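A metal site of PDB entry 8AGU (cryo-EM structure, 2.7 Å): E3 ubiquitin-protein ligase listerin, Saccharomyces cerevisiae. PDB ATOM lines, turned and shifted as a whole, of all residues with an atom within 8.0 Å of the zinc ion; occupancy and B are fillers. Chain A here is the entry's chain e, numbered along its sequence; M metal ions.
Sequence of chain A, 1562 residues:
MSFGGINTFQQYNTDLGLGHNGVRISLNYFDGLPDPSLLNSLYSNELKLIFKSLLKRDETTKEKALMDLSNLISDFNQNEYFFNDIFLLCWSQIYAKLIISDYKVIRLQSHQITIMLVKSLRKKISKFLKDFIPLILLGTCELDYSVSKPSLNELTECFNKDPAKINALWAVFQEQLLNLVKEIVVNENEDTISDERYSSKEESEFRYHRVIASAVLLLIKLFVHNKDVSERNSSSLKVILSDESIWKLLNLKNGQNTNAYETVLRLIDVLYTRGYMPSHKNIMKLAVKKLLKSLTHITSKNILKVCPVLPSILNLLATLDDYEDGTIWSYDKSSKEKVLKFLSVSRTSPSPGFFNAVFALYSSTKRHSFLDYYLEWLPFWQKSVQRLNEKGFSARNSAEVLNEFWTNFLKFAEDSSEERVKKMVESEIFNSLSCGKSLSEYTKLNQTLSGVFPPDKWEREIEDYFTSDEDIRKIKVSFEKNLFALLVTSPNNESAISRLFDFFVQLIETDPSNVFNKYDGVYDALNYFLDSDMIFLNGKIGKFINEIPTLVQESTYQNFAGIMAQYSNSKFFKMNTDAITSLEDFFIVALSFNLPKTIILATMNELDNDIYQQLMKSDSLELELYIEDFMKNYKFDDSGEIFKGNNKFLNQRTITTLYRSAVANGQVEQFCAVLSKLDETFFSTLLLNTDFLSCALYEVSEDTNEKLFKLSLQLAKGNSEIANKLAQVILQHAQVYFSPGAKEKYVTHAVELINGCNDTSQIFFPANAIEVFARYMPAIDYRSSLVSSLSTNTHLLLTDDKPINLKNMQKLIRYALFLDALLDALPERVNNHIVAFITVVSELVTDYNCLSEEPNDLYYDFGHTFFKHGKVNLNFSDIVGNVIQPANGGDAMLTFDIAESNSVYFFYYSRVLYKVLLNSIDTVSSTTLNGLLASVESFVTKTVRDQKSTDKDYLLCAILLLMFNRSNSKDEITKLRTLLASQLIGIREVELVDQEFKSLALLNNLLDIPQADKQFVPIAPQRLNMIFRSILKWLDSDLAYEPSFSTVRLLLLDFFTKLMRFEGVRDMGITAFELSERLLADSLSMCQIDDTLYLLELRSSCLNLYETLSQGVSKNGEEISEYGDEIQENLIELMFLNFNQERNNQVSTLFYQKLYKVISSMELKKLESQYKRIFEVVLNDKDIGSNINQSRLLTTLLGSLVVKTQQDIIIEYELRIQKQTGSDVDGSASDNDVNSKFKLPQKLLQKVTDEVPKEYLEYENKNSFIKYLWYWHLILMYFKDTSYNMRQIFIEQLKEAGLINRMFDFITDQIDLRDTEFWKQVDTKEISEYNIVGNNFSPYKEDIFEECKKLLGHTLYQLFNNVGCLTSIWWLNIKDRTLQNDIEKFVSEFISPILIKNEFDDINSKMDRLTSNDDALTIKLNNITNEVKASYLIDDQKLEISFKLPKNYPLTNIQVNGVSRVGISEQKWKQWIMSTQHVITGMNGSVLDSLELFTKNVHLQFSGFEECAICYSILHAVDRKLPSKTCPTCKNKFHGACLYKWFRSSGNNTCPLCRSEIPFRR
SG of Cys 1508 sits close to N of Ile 1510, at 3.6 Å. N of Cys 1508 lies within hydrogen-bond range of O of Ser 1513 (3.0 Å). A ring nitrogen (ND1) of His 1535 lies close to the side-chain sulfur (SG) of Cys 1511, 3.6 Å away. The backbone carbonyl oxygen of Ser 1513 sits at hydrogen-bond distance from a ring nitrogen (NE2) of His 1535 (3.2 Å). A ring nitrogen (NE2) of His 1535 is in hydrogen-bond range of the backbone carbonyl oxygen of Lys 1521 (3.0 Å). A ring nitrogen (NE2) of His 1535 is in hydrogen-bond range of the backbone carbonyl oxygen (O) of Ile 1514 (2.8 Å). The side-chain sulfur (SG) of Cys 1511 lies within hydrogen-bond range of the side-chain hydroxyl (OG) of Ser 1513, at 3.2 Å.
The zinc ion is bound by SG of Cys 1508, SG of Cys 1538 and ND1 of His 1535. The zinc ion has three donor atoms within binding distance.
Cys 1511 touches the zinc ion. Within 4 Å of the zinc ion: Cys 1508, Cys 1511, His 1535 and Cys 1538.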
ATOM      1  N   GLU A1507      -7.801 -33.464 -22.712  1.00  0.00           N
ATOM      2  CA  GLU A1507      -8.577 -32.640 -23.619  1.00  0.00           C
ATOM      3  C   GLU A1507     -10.007 -33.141 -23.600  1.00  0.00           C
ATOM      4  O   GLU A1507     -10.240 -34.359 -23.588  1.00  0.00           O
ATOM      5  CB  GLU A1507      -8.001 -32.718 -25.031  1.00  0.00           C
ATOM      6  CG  GLU A1507      -6.657 -32.029 -25.183  1.00  0.00           C
ATOM      7  CD  GLU A1507      -6.118 -32.078 -26.598  1.00  0.00           C
ATOM      8  OE1 GLU A1507      -6.591 -32.924 -27.371  1.00  0.00           O
ATOM      9  OE2 GLU A1507      -5.226 -31.271 -26.919  1.00  0.00           O
ATOM     10  N   CYS A1508     -10.968 -32.225 -23.603  1.00  0.00           N
ATOM     11  CA  CYS A1508     -12.363 -32.630 -23.516  1.00  0.00           C
ATOM     12  C   CYS A1508     -12.709 -33.500 -24.703  1.00  0.00           C
ATOM     13  O   CYS A1508     -12.320 -33.189 -25.824  1.00  0.00           O
ATOM     14  CB  CYS A1508     -13.261 -31.403 -23.461  1.00  0.00           C
ATOM     15  SG  CYS A1508     -15.012 -31.719 -23.772  1.00  0.00           S
ATOM     16  N   ALA A1509     -13.450 -34.581 -24.487  1.00  0.00           N
ATOM     17  CA  ALA A1509     -13.742 -35.497 -25.589  1.00  0.00           C
ATOM     18  C   ALA A1509     -14.531 -34.868 -26.728  1.00  0.00           C
ATOM     19  O   ALA A1509     -14.227 -35.106 -27.890  1.00  0.00           O
ATOM     20  CB  ALA A1509     -14.456 -36.732 -25.064  1.00  0.00           C
ATOM     21  N   ILE A1510     -15.542 -34.074 -26.394  1.00  0.00           N
ATOM     22  CA  ILE A1510     -16.389 -33.486 -27.425  1.00  0.00           C
ATOM     23  C   ILE A1510     -15.675 -32.510 -28.363  1.00  0.00           C
ATOM     24  O   ILE A1510     -15.846 -32.584 -29.577  1.00  0.00           O
ATOM     25  CB  ILE A1510     -17.625 -32.816 -26.800  1.00  0.00           C
ATOM     26  CG1 ILE A1510     -18.299 -33.774 -25.807  1.00  0.00           C
ATOM     27  CG2 ILE A1510     -18.618 -32.377 -27.866  1.00  0.00           C
ATOM     28  CD1 ILE A1510     -19.665 -33.319 -25.357  1.00  0.00           C
ATOM     29  N   CYS A1511     -14.856 -31.615 -27.815  1.00  0.00           N
ATOM     30  CA  CYS A1511     -14.172 -30.616 -28.643  1.00  0.00           C
ATOM     31  C   CYS A1511     -12.668 -30.820 -28.802  1.00  0.00           C
ATOM     32  O   CYS A1511     -12.007 -30.012 -29.456  1.00  0.00           O
ATOM     33  CB  CYS A1511     -14.447 -29.214 -28.107  1.00  0.00           C
ATOM     34  SG  CYS A1511     -13.889 -28.954 -26.409  1.00  0.00           S
ATOM     35  N   TYR A1512     -12.119 -31.862 -28.184  1.00  0.00           N
ATOM     36  CA  TYR A1512     -10.676 -32.149 -28.267  1.00  0.00           C
ATOM     37  C   TYR A1512      -9.789 -31.004 -27.793  1.00  0.00           C
ATOM     38  O   TYR A1512      -8.723 -30.765 -28.358  1.00  0.00           O
ATOM     39  CB  TYR A1512     -10.282 -32.640 -29.664  1.00  0.00           C
ATOM     40  CG  TYR A1512      -9.158 -33.654 -29.649  1.00  0.00           C
ATOM     41  CD1 TYR A1512      -9.225 -34.776 -28.826  1.00  0.00           C
ATOM     42  CD2 TYR A1512      -8.047 -33.498 -30.457  1.00  0.00           C
ATOM     43  CE1 TYR A1512      -8.209 -35.711 -28.814  1.00  0.00           C
ATOM     44  CE2 TYR A1512      -7.020 -34.430 -30.445  1.00  0.00           C
ATOM     45  CZ  TYR A1512      -7.103 -35.527 -29.619  1.00  0.00           C
ATOM     46  OH  TYR A1512      -6.088 -36.454 -29.613  1.00  0.00           O
ATOM     47  N   SER A1513     -10.217 -30.283 -26.756  1.00  0.00           N
ATOM     48  CA  SER A1513      -9.382 -29.219 -26.206  1.00  0.00           C
ATOM     49  C   SER A1513      -9.479 -29.154 -24.697  1.00  0.00           C
ATOM     50  O   SER A1513     -10.565 -29.352 -24.142  1.00  0.00           O
ATOM     51  CB  SER A1513      -9.769 -27.863 -26.808  1.00  0.00           C
ATOM     52  OG  SER A1513     -11.062 -27.477 -26.410  1.00  0.00           O
ATOM     53  N   ILE A1514      -8.380 -28.857 -24.012  1.00  0.00           N
ATOM     54  CA  ILE A1514      -8.440 -28.687 -22.564  1.00  0.00           C
ATOM     55  C   ILE A1514      -9.311 -27.486 -22.271  1.00  0.00           C
ATOM     56  O   ILE A1514     -10.136 -27.513 -21.368  1.00  0.00           O
ATOM     57  CB  ILE A1514      -7.035 -28.460 -21.967  1.00  0.00           C
ATOM     58  CG1 ILE A1514      -6.098 -29.605 -22.338  1.00  0.00           C
ATOM     59  CG2 ILE A1514      -7.112 -28.341 -20.449  1.00  0.00           C
ATOM     60  CD1 ILE A1514      -4.742 -29.523 -21.676  1.00  0.00           C
ATOM     61  N   LEU A1515      -9.146 -26.433 -23.063  1.00  0.00           N
ATOM     62  CA  LEU A1515      -9.969 -25.243 -22.887  1.00  0.00           C
ATOM     63  C   LEU A1515     -10.678 -24.899 -24.169  1.00  0.00           C
ATOM     64  O   LEU A1515     -10.044 -24.819 -25.220  1.00  0.00           O
ATOM     65  CB  LEU A1515      -9.109 -24.045 -22.515  1.00  0.00           C
ATOM     66  CG  LEU A1515      -8.117 -24.101 -21.354  1.00  0.00           C
ATOM     67  CD1 LEU A1515      -7.215 -22.875 -21.438  1.00  0.00           C
ATOM     68  CD2 LEU A1515      -8.843 -24.162 -20.026  1.00  0.00           C
ATOM     69  N   HIS A1516     -11.990 -24.664 -24.120  1.00  0.00           N
ATOM     70  CA  HIS A1516     -12.676 -24.206 -25.311  1.00  0.00           C
ATOM     71  C   HIS A1516     -12.098 -22.813 -25.498  1.00  0.00           C
ATOM     72  O   HIS A1516     -11.871 -22.117 -24.519  1.00  0.00           O
ATOM     73  CB  HIS A1516     -14.182 -24.117 -25.066  1.00  0.00           C
ATOM     74  CG  HIS A1516     -14.979 -23.774 -26.279  1.00  0.00           C
ATOM     75  ND1 HIS A1516     -15.142 -22.479 -26.736  1.00  0.00           N
ATOM     76  CD2 HIS A1516     -15.674 -24.555 -27.147  1.00  0.00           C
ATOM     77  CE1 HIS A1516     -15.892 -22.482 -27.816  1.00  0.00           C
ATOM     78  NE2 HIS A1516     -16.226 -23.735 -28.091  1.00  0.00           N
ATOM     79  N   ASP A1519     -14.704 -20.475 -24.314  1.00  0.00           N
ATOM     80  CA  ASP A1519     -15.038 -20.844 -22.938  1.00  0.00           C
ATOM     81  C   ASP A1519     -13.929 -20.707 -21.915  1.00  0.00           C
ATOM     82  O   ASP A1519     -14.182 -20.276 -20.793  1.00  0.00           O
ATOM     83  CB  ASP A1519     -15.616 -22.270 -22.895  1.00  0.00           C
ATOM     84  CG  ASP A1519     -16.910 -22.389 -23.677  1.00  0.00           C
ATOM     85  OD1 ASP A1519     -17.296 -21.411 -24.352  1.00  0.00           O
ATOM     86  OD2 ASP A1519     -17.536 -23.471 -23.617  1.00  0.00           O
ATOM     87  N   LYS A1521     -12.558 -23.022 -20.263  1.00  0.00           N
ATOM     88  CA  LYS A1521     -12.983 -23.805 -19.112  1.00  0.00           C
ATOM     89  C   LYS A1521     -12.338 -25.170 -19.067  1.00  0.00           C
ATOM     90  O   LYS A1521     -12.291 -25.867 -20.077  1.00  0.00           O
ATOM     91  CB  LYS A1521     -14.507 -23.948 -19.107  1.00  0.00           C
ATOM     92  CG  LYS A1521     -15.070 -24.579 -17.853  1.00  0.00           C
ATOM     93  CD  LYS A1521     -16.569 -24.761 -17.930  1.00  0.00           C
ATOM     94  CE  LYS A1521     -17.116 -25.362 -16.647  1.00  0.00           C
ATOM     95  NZ  LYS A1521     -18.605 -25.481 -16.671  1.00  0.00           N
ATOM     96  N   LEU A1522     -11.840 -25.562 -17.902  1.00  0.00           N
ATOM     97  CA  LEU A1522     -11.230 -26.870 -17.737  1.00  0.00           C
ATOM     98  C   LEU A1522     -12.260 -27.969 -17.843  1.00  0.00           C
ATOM     99  O   LEU A1522     -13.426 -27.765 -17.472  1.00  0.00           O
ATOM    100  CB  LEU A1522     -10.549 -26.958 -16.373  1.00  0.00           C
ATOM    101  CG  LEU A1522      -9.328 -26.073 -16.179  1.00  0.00           C
ATOM    102  CD1 LEU A1522      -8.901 -26.089 -14.723  1.00  0.00           C
ATOM    103  CD2 LEU A1522      -8.202 -26.521 -17.088  1.00  0.00           C
ATOM    104  N   PRO A1523     -11.864 -29.149 -18.331  1.00  0.00           N
ATOM    105  CA  PRO A1523     -12.815 -30.260 -18.352  1.00  0.00           C
ATOM    106  C   PRO A1523     -12.782 -30.932 -16.989  1.00  0.00           C
ATOM    107  O   PRO A1523     -12.247 -32.035 -16.864  1.00  0.00           O
ATOM    108  CB  PRO A1523     -12.252 -31.205 -19.418  1.00  0.00           C
ATOM    109  CG  PRO A1523     -11.012 -30.552 -19.948  1.00  0.00           C
ATOM    110  CD  PRO A1523     -10.585 -29.522 -18.955  1.00  0.00           C
ATOM    111  N   LYS A1533     -11.766 -36.842 -20.169  1.00  0.00           N
ATOM    112  CA  LYS A1533     -12.451 -35.783 -19.414  1.00  0.00           C
ATOM    113  C   LYS A1533     -13.460 -35.003 -20.260  1.00  0.00           C
ATOM    114  O   LYS A1533     -13.380 -35.012 -21.487  1.00  0.00           O
ATOM    115  CB  LYS A1533     -11.437 -34.826 -18.790  1.00  0.00           C
ATOM    116  CG  LYS A1533     -10.598 -35.463 -17.704  1.00  0.00           C
ATOM    117  CD  LYS A1533      -9.888 -34.408 -16.870  1.00  0.00           C
ATOM    118  CE  LYS A1533      -9.152 -35.021 -15.698  1.00  0.00           C
ATOM    119  NZ  LYS A1533      -8.647 -33.986 -14.752  1.00  0.00           N
ATOM    120  N   PHE A1534     -14.407 -34.342 -19.605  1.00  0.00           N
ATOM    121  CA  PHE A1534     -15.392 -33.545 -20.316  1.00  0.00           C
ATOM    122  C   PHE A1534     -15.481 -32.145 -19.742  1.00  0.00           C
ATOM    123  O   PHE A1534     -15.292 -31.958 -18.543  1.00  0.00           O
ATOM    124  CB  PHE A1534     -16.783 -34.168 -20.214  1.00  0.00           C
ATOM    125  CG  PHE A1534     -16.821 -35.632 -20.549  1.00  0.00           C
ATOM    126  CD1 PHE A1534     -16.765 -36.052 -21.863  1.00  0.00           C
ATOM    127  CD2 PHE A1534     -16.936 -36.575 -19.542  1.00  0.00           C
ATOM    128  CE1 PHE A1534     -16.806 -37.396 -22.170  1.00  0.00           C
ATOM    129  CE2 PHE A1534     -16.977 -37.919 -19.848  1.00  0.00           C
ATOM    130  CZ  PHE A1534     -16.913 -38.323 -21.161  1.00  0.00           C
ATOM    131  N   HIS A1535     -15.755 -31.155 -20.587  1.00  0.00           N
ATOM    132  CA  HIS A1535     -15.969 -29.811 -20.073  1.00  0.00           C
ATOM    133  C   HIS A1535     -17.243 -29.870 -19.263  1.00  0.00           C
ATOM    134  O   HIS A1535     -18.163 -30.612 -19.610  1.00  0.00           O
ATOM    135  CB  HIS A1535     -16.111 -28.795 -21.201  1.00  0.00           C
ATOM    136  CG  HIS A1535     -14.818 -28.371 -21.806  1.00  0.00           C
ATOM    137  ND1 HIS A1535     -14.729 -27.827 -23.070  1.00  0.00           N
ATOM    138  CD2 HIS A1535     -13.550 -28.408 -21.329  1.00  0.00           C
ATOM    139  CE1 HIS A1535     -13.462 -27.542 -23.334  1.00  0.00           C
ATOM    140  NE2 HIS A1535     -12.734 -27.894 -22.295  1.00  0.00           N
ATOM    141  N   GLY A1536     -17.320 -29.105 -18.182  1.00  0.00           N
ATOM    142  CA  GLY A1536     -18.484 -29.189 -17.323  1.00  0.00           C
ATOM    143  C   GLY A1536     -19.760 -28.824 -18.056  1.00  0.00           C
ATOM    144  O   GLY A1536     -20.767 -29.523 -17.934  1.00  0.00           O
ATOM    145  N   ALA A1537     -19.721 -27.754 -18.839  1.00  0.00           N
ATOM    146  CA  ALA A1537     -20.890 -27.378 -19.620  1.00  0.00           C
ATOM    147  C   ALA A1537     -21.238 -28.455 -20.657  1.00  0.00           C
ATOM    148  O   ALA A1537     -22.412 -28.759 -20.855  1.00  0.00           O
ATOM    149  CB  ALA A1537     -20.666 -26.034 -20.298  1.00  0.00           C
ATOM    150  N   CYS A1538     -20.217 -29.022 -21.304  1.00  0.00           N
ATOM    151  CA  CYS A1538     -20.466 -30.029 -22.322  1.00  0.00           C
ATOM    152  C   CYS A1538     -21.140 -31.235 -21.699  1.00  0.00           C
ATOM    153  O   CYS A1538     -22.125 -31.759 -22.242  1.00  0.00           O
ATOM    154  CB  CYS A1538     -19.134 -30.469 -22.975  1.00  0.00           C
ATOM    155  SG  CYS A1538     -18.303 -29.238 -24.011  1.00  0.00           S
ATOM    156  N   LEU A1539     -20.654 -31.673 -20.536  1.00  0.00           N
ATOM    157  CA  LEU A1539     -21.245 -32.816 -19.850  1.00  0.00           C
ATOM    158  C   LEU A1539     -22.669 -32.530 -19.407  1.00  0.00           C
ATOM    159  O   LEU A1539     -23.550 -33.371 -19.586  1.00  0.00           O
ATOM    160  CB  LEU A1539     -20.378 -33.203 -18.645  1.00  0.00           C
ATOM    161  CG  LEU A1539     -20.915 -34.308 -17.733  1.00  0.00           C
ATOM    162  CD1 LEU A1539     -19.933 -35.452 -17.625  1.00  0.00           C
ATOM    163  CD2 LEU A1539     -21.272 -33.750 -16.363  1.00  0.00           C
HETATM  164 ZN    ZN M   1     -15.994 -29.637 -24.171  1.00  0.00          ZN
